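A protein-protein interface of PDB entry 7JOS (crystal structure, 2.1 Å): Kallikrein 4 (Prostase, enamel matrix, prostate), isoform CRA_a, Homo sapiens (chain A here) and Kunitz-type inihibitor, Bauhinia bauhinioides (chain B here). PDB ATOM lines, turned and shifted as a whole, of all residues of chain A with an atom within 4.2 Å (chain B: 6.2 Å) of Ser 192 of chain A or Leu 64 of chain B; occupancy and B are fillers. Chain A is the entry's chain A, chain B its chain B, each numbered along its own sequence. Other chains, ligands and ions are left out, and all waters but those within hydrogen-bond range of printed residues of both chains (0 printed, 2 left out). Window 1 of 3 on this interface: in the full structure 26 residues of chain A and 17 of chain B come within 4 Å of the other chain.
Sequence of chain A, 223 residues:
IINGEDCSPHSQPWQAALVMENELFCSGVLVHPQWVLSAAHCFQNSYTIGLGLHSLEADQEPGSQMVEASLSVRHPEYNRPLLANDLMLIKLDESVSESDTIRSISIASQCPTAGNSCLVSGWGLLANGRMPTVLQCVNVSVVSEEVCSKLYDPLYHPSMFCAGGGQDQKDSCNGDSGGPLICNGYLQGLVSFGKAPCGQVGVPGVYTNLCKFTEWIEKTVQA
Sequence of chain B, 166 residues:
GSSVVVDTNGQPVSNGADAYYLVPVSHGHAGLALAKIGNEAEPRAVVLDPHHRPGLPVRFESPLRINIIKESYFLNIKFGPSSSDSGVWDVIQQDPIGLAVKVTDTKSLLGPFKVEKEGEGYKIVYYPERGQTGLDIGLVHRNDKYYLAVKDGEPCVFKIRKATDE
The side-chain hydroxyl of Ser 177 of chain A sits at hydrogen-bond distance from the backbone NH of Ile 66 of chain B, 3.2 Å away.
O of Ser 192 of chain A lies within hydrogen-bond range of N of Arg 65 of chain B (3.1 Å).
The side-chain hydroxyl (OG) of Ser 177 of chain A sits close to the backbone carbonyl oxygen (O) of Arg 65 of chain B, at 2.9 Å.
The side-chain hydroxyl of Tyr 73 of chain B sits at hydrogen-bond distance from the backbone carbonyl oxygen of His 41 of chain A (2.7 Å).
The side-chain amide nitrogen (ND2) of Asn 174 of chain A is in hydrogen-bond range of the backbone carbonyl oxygen (O) of Asn 15 of chain B (3.3 Å).
The side-chain amide nitrogen (ND2) of Asn 15 of chain B is in hydrogen-bond range of the backbone carbonyl oxygen (O) of Ile 66 of chain B (3.0 Å).
The backbone NH (N) of Leu 64 of chain B sits close to the side-chain hydroxyl (OG) of Ser 62 of chain B, at 3.2 Å.
O of Val 206 of chain A lies within hydrogen-bond range of N of Ser 192 of chain A, 3.1 Å away.
A ring nitrogen (ND1) of His 41 of chain A sits at hydrogen-bond distance from the side-chain carboxylate (OD2) of Asp 86 of chain A (2.8 Å).
The side-chain carboxylate of Asp 86 of chain A sits at hydrogen-bond distance from the side-chain hydroxyl of Ser 192 of chain A (2.7 Å).
The side-chain hydroxyl of Ser 177 of chain A is in hydrogen-bond range of a ring nitrogen (NE2) of His 41 of chain A (2.7 Å).
Among the printed residues, pairs that only touch across the chains: Phe 193 of chain A with Pro 63 of chain B (3.3 Å), Asn 174 of chain A with Arg 65 of chain B (3.5 Å), Asn 174 of chain A with Ile 66 of chain B (3.5 Å), Ser 192 of chain A with Leu 64 of chain B (3.6 Å), Val 191 of chain A with Arg 65 of chain B (3.7 Å), His 41 of chain A with Leu 64 of chain B (3.7 Å), Asn 174 of chain A with Leu 64 of chain B (3.7 Å), Phe 193 of chain A with Leu 64 of chain B (3.8 Å), Phe 193 of chain A with Arg 65 of chain B (3.9 Å), His 41 of chain A with Ile 66 of chain B (3.96 Å) and Leu 83 of chain A with Leu 64 of chain B (3.98 Å).
Ser 192 of chain A touches just these residues of chain B: Leu 64 (3.6 Å) and Arg 65 (3.1 Å).
Of the printed residues of chain A, Leu 64 of chain B touches His 41 (3.7 Å), Leu 83 (3.98 Å), Asn 174 (3.7 Å), Ser 192 (3.6 Å) and Phe 193 (3.8 Å).
Printed residues of chain A within 4 Å of Ile 66 of chain B: His 41, Asn 174 and Ser 177.
Printed residues of chain B within 4 Å of Leu 83 of chain A: Leu 64.
Of the printed residues of chain B, His 41 of chain A touches Leu 64, Ile 66 and Tyr 73.
Of the printed residues of chain A, Arg 65 of chain B touches Asn 174 (3.5 Å), Ser 177 (2.8 Å), Val 191 (3.7 Å), Ser 192 (3.1 Å) and Phe 193 (3.9 Å).
Ser 62 of chain B touches none of the printed residues of chain A.
Asn 67 of chain B touches none of the printed residues of chain A.
The nearest residue of chain B that does not touch Ser 192 of chain A is Pro 63 of chain B (4.6 Å).
The nearest printed residue of chain B that does not touch His 41 of chain A is Arg 65 of chain B (4.2 Å).
Hydrophobic or aromatic side chains of chain A within 4 Å of the printed part of chain B: His 41, Leu 83, Val 191 and Phe 193.
Of the 8 printed residues of chain B, 6 touch a printed residue of chain A.
Hydrophobic or aromatic side chains of chain B within 4 Å of the printed part of chain A: Leu 64, Ile 66 and Tyr 73.
Among the printed residues, 16 pairs touch across the chains.
Among the printed residues, no Asp or Glu carboxylate lies within 4 Å of a Lys or Arg side-chain nitrogen of the other chain.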
ATOM      1  N   HIS A  41      27.675 -10.279 -24.601  1.00  0.00           N
ATOM      2  CA  HIS A  41      26.613  -9.679 -25.445  1.00  0.00           C
ATOM      3  C   HIS A  41      25.289  -9.621 -24.679  1.00  0.00           C
ATOM      4  O   HIS A  41      24.352  -8.971 -25.194  1.00  0.00           O
ATOM      5  CB  HIS A  41      26.492 -10.401 -26.785  1.00  0.00           C
ATOM      6  CG  HIS A  41      25.866 -11.754 -26.754  1.00  0.00           C
ATOM      7  ND1 HIS A  41      26.616 -12.918 -26.768  1.00  0.00           N
ATOM      8  CD2 HIS A  41      24.574 -12.133 -26.760  1.00  0.00           C
ATOM      9  CE1 HIS A  41      25.799 -13.945 -26.731  1.00  0.00           C
ATOM     10  NE2 HIS A  41      24.554 -13.499 -26.735  1.00  0.00           N
ATOM     11  N   LEU A  83      32.888 -10.807 -32.237  1.00  0.00           N
ATOM     12  CA  LEU A  83      32.269 -12.004 -31.629  1.00  0.00           C
ATOM     13  C   LEU A  83      33.212 -12.707 -30.651  1.00  0.00           C
ATOM     14  O   LEU A  83      32.725 -13.589 -29.902  1.00  0.00           O
ATOM     15  CB  LEU A  83      31.821 -12.976 -32.719  1.00  0.00           C
ATOM     16  CG  LEU A  83      30.805 -12.449 -33.724  1.00  0.00           C
ATOM     17  CD1 LEU A  83      30.303 -13.603 -34.578  1.00  0.00           C
ATOM     18  CD2 LEU A  83      29.635 -11.785 -33.015  1.00  0.00           C
ATOM     19  N   ASP A  86      33.779 -13.521 -25.702  1.00  0.00           N
ATOM     20  CA  ASP A  86      32.369 -13.247 -25.331  1.00  0.00           C
ATOM     21  C   ASP A  86      32.097 -13.751 -23.913  1.00  0.00           C
ATOM     22  O   ASP A  86      31.424 -14.800 -23.767  1.00  0.00           O
ATOM     23  CB  ASP A  86      31.451 -13.865 -26.386  1.00  0.00           C
ATOM     24  CG  ASP A  86      30.008 -13.400 -26.271  1.00  0.00           C
ATOM     25  OD1 ASP A  86      29.726 -12.511 -25.425  1.00  0.00           O
ATOM     26  OD2 ASP A  86      29.168 -13.945 -27.023  1.00  0.00           O
ATOM     27  N   ASN A 174      18.013 -19.319 -29.565  1.00  0.00           N
ATOM     28  CA  ASN A 174      17.820 -17.951 -29.048  1.00  0.00           C
ATOM     29  C   ASN A 174      17.191 -17.998 -27.650  1.00  0.00           C
ATOM     30  O   ASN A 174      16.176 -18.658 -27.479  1.00  0.00           O
ATOM     31  CB  ASN A 174      17.029 -17.125 -30.060  1.00  0.00           C
ATOM     32  CG  ASN A 174      17.814 -16.867 -31.330  1.00  0.00           C
ATOM     33  OD1 ASN A 174      19.002 -17.174 -31.410  1.00  0.00           O
ATOM     34  ND2 ASN A 174      17.167 -16.307 -32.326  1.00  0.00           N
ATOM     35  N   SER A 177      21.858 -18.061 -24.950  1.00  0.00           N
ATOM     36  CA  SER A 177      23.112 -17.289 -24.746  1.00  0.00           C
ATOM     37  C   SER A 177      23.485 -17.218 -23.257  1.00  0.00           C
ATOM     38  O   SER A 177      22.616 -16.929 -22.427  1.00  0.00           O
ATOM     39  CB  SER A 177      22.983 -15.883 -25.291  1.00  0.00           C
ATOM     40  OG  SER A 177      23.273 -15.830 -26.672  1.00  0.00           O
ATOM     41  N   LEU A 190      30.394 -21.231 -22.629  1.00  0.00           N
ATOM     42  CA  LEU A 190      29.118 -20.488 -22.564  1.00  0.00           C
ATOM     43  C   LEU A 190      28.525 -20.473 -23.976  1.00  0.00           C
ATOM     44  O   LEU A 190      29.281 -20.289 -24.925  1.00  0.00           O
ATOM     45  CB  LEU A 190      29.337 -19.046 -22.100  1.00  0.00           C
ATOM     46  CG  LEU A 190      30.063 -18.852 -20.783  1.00  0.00           C
ATOM     47  CD1 LEU A 190      30.424 -17.385 -20.571  1.00  0.00           C
ATOM     48  CD2 LEU A 190      29.200 -19.354 -19.630  1.00  0.00           C
ATOM     49  N   VAL A 191      27.215 -20.668 -24.080  1.00  0.00           N
ATOM     50  CA  VAL A 191      26.511 -20.440 -25.358  1.00  0.00           C
ATOM     51  C   VAL A 191      26.810 -19.031 -25.845  1.00  0.00           C
ATOM     52  O   VAL A 191      26.580 -18.086 -25.101  1.00  0.00           O
ATOM     53  CB  VAL A 191      25.000 -20.654 -25.194  1.00  0.00           C
ATOM     54  CG1 VAL A 191      24.269 -20.423 -26.506  1.00  0.00           C
ATOM     55  CG2 VAL A 191      24.675 -22.035 -24.651  1.00  0.00           C
ATOM     56  N   SER A 192      27.299 -18.912 -27.081  1.00  0.00           N
ATOM     57  CA  SER A 192      27.695 -17.586 -27.617  1.00  0.00           C
ATOM     58  C   SER A 192      26.910 -17.312 -28.900  1.00  0.00           C
ATOM     59  O   SER A 192      26.004 -16.466 -28.876  1.00  0.00           O
ATOM     60  CB  SER A 192      29.198 -17.527 -27.805  1.00  0.00           C
ATOM     61  OG  SER A 192      29.599 -16.281 -28.357  1.00  0.00           O
ATOM     62  N   PHE A 193      27.185 -18.056 -29.967  1.00  0.00           N
ATOM     63  CA  PHE A 193      26.496 -17.748 -31.240  1.00  0.00           C
ATOM     64  C   PHE A 193      26.525 -18.970 -32.137  1.00  0.00           C
ATOM     65  O   PHE A 193      27.154 -19.985 -31.793  1.00  0.00           O
ATOM     66  CB  PHE A 193      27.159 -16.559 -31.932  1.00  0.00           C
ATOM     67  CG  PHE A 193      28.532 -16.814 -32.495  1.00  0.00           C
ATOM     68  CD1 PHE A 193      29.662 -16.555 -31.749  1.00  0.00           C
ATOM     69  CD2 PHE A 193      28.684 -17.229 -33.808  1.00  0.00           C
ATOM     70  CE1 PHE A 193      30.932 -16.758 -32.284  1.00  0.00           C
ATOM     71  CE2 PHE A 193      29.949 -17.400 -34.350  1.00  0.00           C
ATOM     72  CZ  PHE A 193      31.066 -17.185 -33.590  1.00  0.00           C
ATOM     73  N   VAL A 206      28.626 -22.229 -31.522  1.00  0.00           N
ATOM     74  CA  VAL A 206      29.903 -21.687 -30.997  1.00  0.00           C
ATOM     75  C   VAL A 206      29.723 -21.317 -29.531  1.00  0.00           C
ATOM     76  O   VAL A 206      28.681 -20.739 -29.167  1.00  0.00           O
ATOM     77  CB  VAL A 206      30.400 -20.499 -31.821  1.00  0.00           C
ATOM     78  CG1 VAL A 206      31.798 -20.069 -31.381  1.00  0.00           C
ATOM     79  CG2 VAL A 206      30.402 -20.851 -33.293  1.00  0.00           C
ATOM     80  N   THR A 208      31.897 -19.875 -25.903  1.00  0.00           N
ATOM     81  CA  THR A 208      33.076 -19.161 -25.370  1.00  0.00           C
ATOM     82  C   THR A 208      34.038 -20.189 -24.777  1.00  0.00           C
ATOM     83  O   THR A 208      33.595 -21.023 -23.947  1.00  0.00           O
ATOM     84  CB  THR A 208      32.655 -18.132 -24.321  1.00  0.00           C
ATOM     85  OG1 THR A 208      31.672 -17.302 -24.934  1.00  0.00           O
ATOM     86  CG2 THR A 208      33.814 -17.290 -23.840  1.00  0.00           C
ATOM     87  N   ASN B  15      15.193 -11.138 -32.284  1.00  0.00           N
ATOM     88  CA  ASN B  15      16.288 -11.587 -33.176  1.00  0.00           C
ATOM     89  C   ASN B  15      15.717 -12.595 -34.162  1.00  0.00           C
ATOM     90  O   ASN B  15      15.662 -13.762 -33.821  1.00  0.00           O
ATOM     91  CB  ASN B  15      17.426 -12.175 -32.334  1.00  0.00           C
ATOM     92  CG  ASN B  15      18.605 -12.613 -33.173  1.00  0.00           C
ATOM     93  OD1 ASN B  15      18.612 -12.397 -34.398  1.00  0.00           O
ATOM     94  ND2 ASN B  15      19.600 -13.187 -32.515  1.00  0.00           N
ATOM     95  N   SER B  62      20.834 -11.581 -35.873  1.00  0.00           N
ATOM     96  CA  SER B  62      22.200 -11.698 -35.326  1.00  0.00           C
ATOM     97  C   SER B  62      22.485 -13.168 -35.095  1.00  0.00           C
ATOM     98  O   SER B  62      21.608 -13.902 -34.642  1.00  0.00           O
ATOM     99  CB  SER B  62      22.294 -10.941 -34.011  1.00  0.00           C
ATOM    100  OG  SER B  62      23.522 -11.204 -33.367  1.00  0.00           O
ATOM    101  N   PRO B  63      23.735 -13.637 -35.304  1.00  0.00           N
ATOM    102  CA  PRO B  63      24.081 -15.023 -34.980  1.00  0.00           C
ATOM    103  C   PRO B  63      24.118 -15.283 -33.463  1.00  0.00           C
ATOM    104  O   PRO B  63      24.050 -16.430 -33.058  1.00  0.00           O
ATOM    105  CB  PRO B  63      25.466 -15.174 -35.621  1.00  0.00           C
ATOM    106  CG  PRO B  63      26.024 -13.794 -35.616  1.00  0.00           C
ATOM    107  CD  PRO B  63      24.856 -12.878 -35.855  1.00  0.00           C
ATOM    108  N   LEU B  64      24.219 -14.217 -32.660  1.00  0.00           N
ATOM    109  CA  LEU B  64      24.195 -14.342 -31.177  1.00  0.00           C
ATOM    110  C   LEU B  64      22.948 -15.097 -30.728  1.00  0.00           C
ATOM    111  O   LEU B  64      21.877 -14.804 -31.301  1.00  0.00           O
ATOM    112  CB  LEU B  64      24.216 -12.938 -30.565  1.00  0.00           C
ATOM    113  CG  LEU B  64      25.428 -12.088 -30.949  1.00  0.00           C
ATOM    114  CD1 LEU B  64      25.297 -10.685 -30.380  1.00  0.00           C
ATOM    115  CD2 LEU B  64      26.718 -12.727 -30.470  1.00  0.00           C
ATOM    116  N   ARG B  65      23.080 -15.987 -29.726  1.00  0.00           N
ATOM    117  CA  ARG B  65      21.926 -16.825 -29.306  1.00  0.00           C
ATOM    118  C   ARG B  65      21.050 -16.088 -28.287  1.00  0.00           C
ATOM    119  O   ARG B  65      20.568 -16.734 -27.341  1.00  0.00           O
ATOM    120  CB  ARG B  65      22.422 -18.162 -28.739  1.00  0.00           C
ATOM    121  CG  ARG B  65      23.086 -19.065 -29.755  1.00  0.00           C
ATOM    122  CD  ARG B  65      22.286 -19.159 -31.018  1.00  0.00           C
ATOM    123  NE  ARG B  65      22.545 -20.376 -31.772  1.00  0.00           N
ATOM    124  CZ  ARG B  65      22.516 -20.434 -33.094  1.00  0.00           C
ATOM    125  NH1 ARG B  65      22.256 -19.341 -33.824  1.00  0.00           N
ATOM    126  NH2 ARG B  65      22.774 -21.590 -33.674  1.00  0.00           N
ATOM    127  N   ILE B  66      20.856 -14.798 -28.493  1.00  0.00           N
ATOM    128  CA  ILE B  66      19.936 -13.977 -27.647  1.00  0.00           C
ATOM    129  C   ILE B  66      18.652 -13.738 -28.466  1.00  0.00           C
ATOM    130  O   ILE B  66      18.686 -13.866 -29.706  1.00  0.00           O
ATOM    131  CB  ILE B  66      20.674 -12.689 -27.250  1.00  0.00           C
ATOM    132  CG1 ILE B  66      19.901 -11.921 -26.177  1.00  0.00           C
ATOM    133  CG2 ILE B  66      21.025 -11.855 -28.488  1.00  0.00           C
ATOM    134  CD1 ILE B  66      20.718 -10.796 -25.561  1.00  0.00           C
ATOM    135  N   ASN B  67      17.533 -13.458 -27.799  1.00  0.00           N
ATOM    136  CA  ASN B  67      16.213 -13.359 -28.470  1.00  0.00           C
ATOM    137  C   ASN B  67      15.836 -11.886 -28.691  1.00  0.00           C
ATOM    138  O   ASN B  67      14.732 -11.632 -29.162  1.00  0.00           O
ATOM    139  CB  ASN B  67      15.136 -14.127 -27.699  1.00  0.00           C
ATOM    140  CG  ASN B  67      14.996 -13.718 -26.233  1.00  0.00           C
ATOM    141  OD1 ASN B  67      14.282 -14.340 -25.458  1.00  0.00           O
ATOM    142  ND2 ASN B  67      15.687 -12.671 -25.810  1.00  0.00           N
ATOM    143  N   TYR B  73      24.720  -4.431 -32.020  1.00  0.00           N
ATOM    144  CA  TYR B  73      24.845  -5.683 -32.812  1.00  0.00           C
ATOM    145  C   TYR B  73      24.921  -5.413 -34.318  1.00  0.00           C
ATOM    146  O   TYR B  73      24.141  -4.600 -34.877  1.00  0.00           O
ATOM    147  CB  TYR B  73      23.655  -6.605 -32.594  1.00  0.00           C
ATOM    148  CG  TYR B  73      23.459  -7.145 -31.194  1.00  0.00           C
ATOM    149  CD1 TYR B  73      24.419  -7.023 -30.201  1.00  0.00           C
ATOM    150  CD2 TYR B  73      22.326  -7.861 -30.891  1.00  0.00           C
ATOM    151  CE1 TYR B  73      24.231  -7.554 -28.935  1.00  0.00           C
ATOM    152  CE2 TYR B  73      22.126  -8.406 -29.631  1.00  0.00           C
ATOM    153  CZ  TYR B  73      23.072  -8.242 -28.647  1.00  0.00           C
ATOM    154  OH  TYR B  73      22.812  -8.785 -27.419  1.00  0.00           O
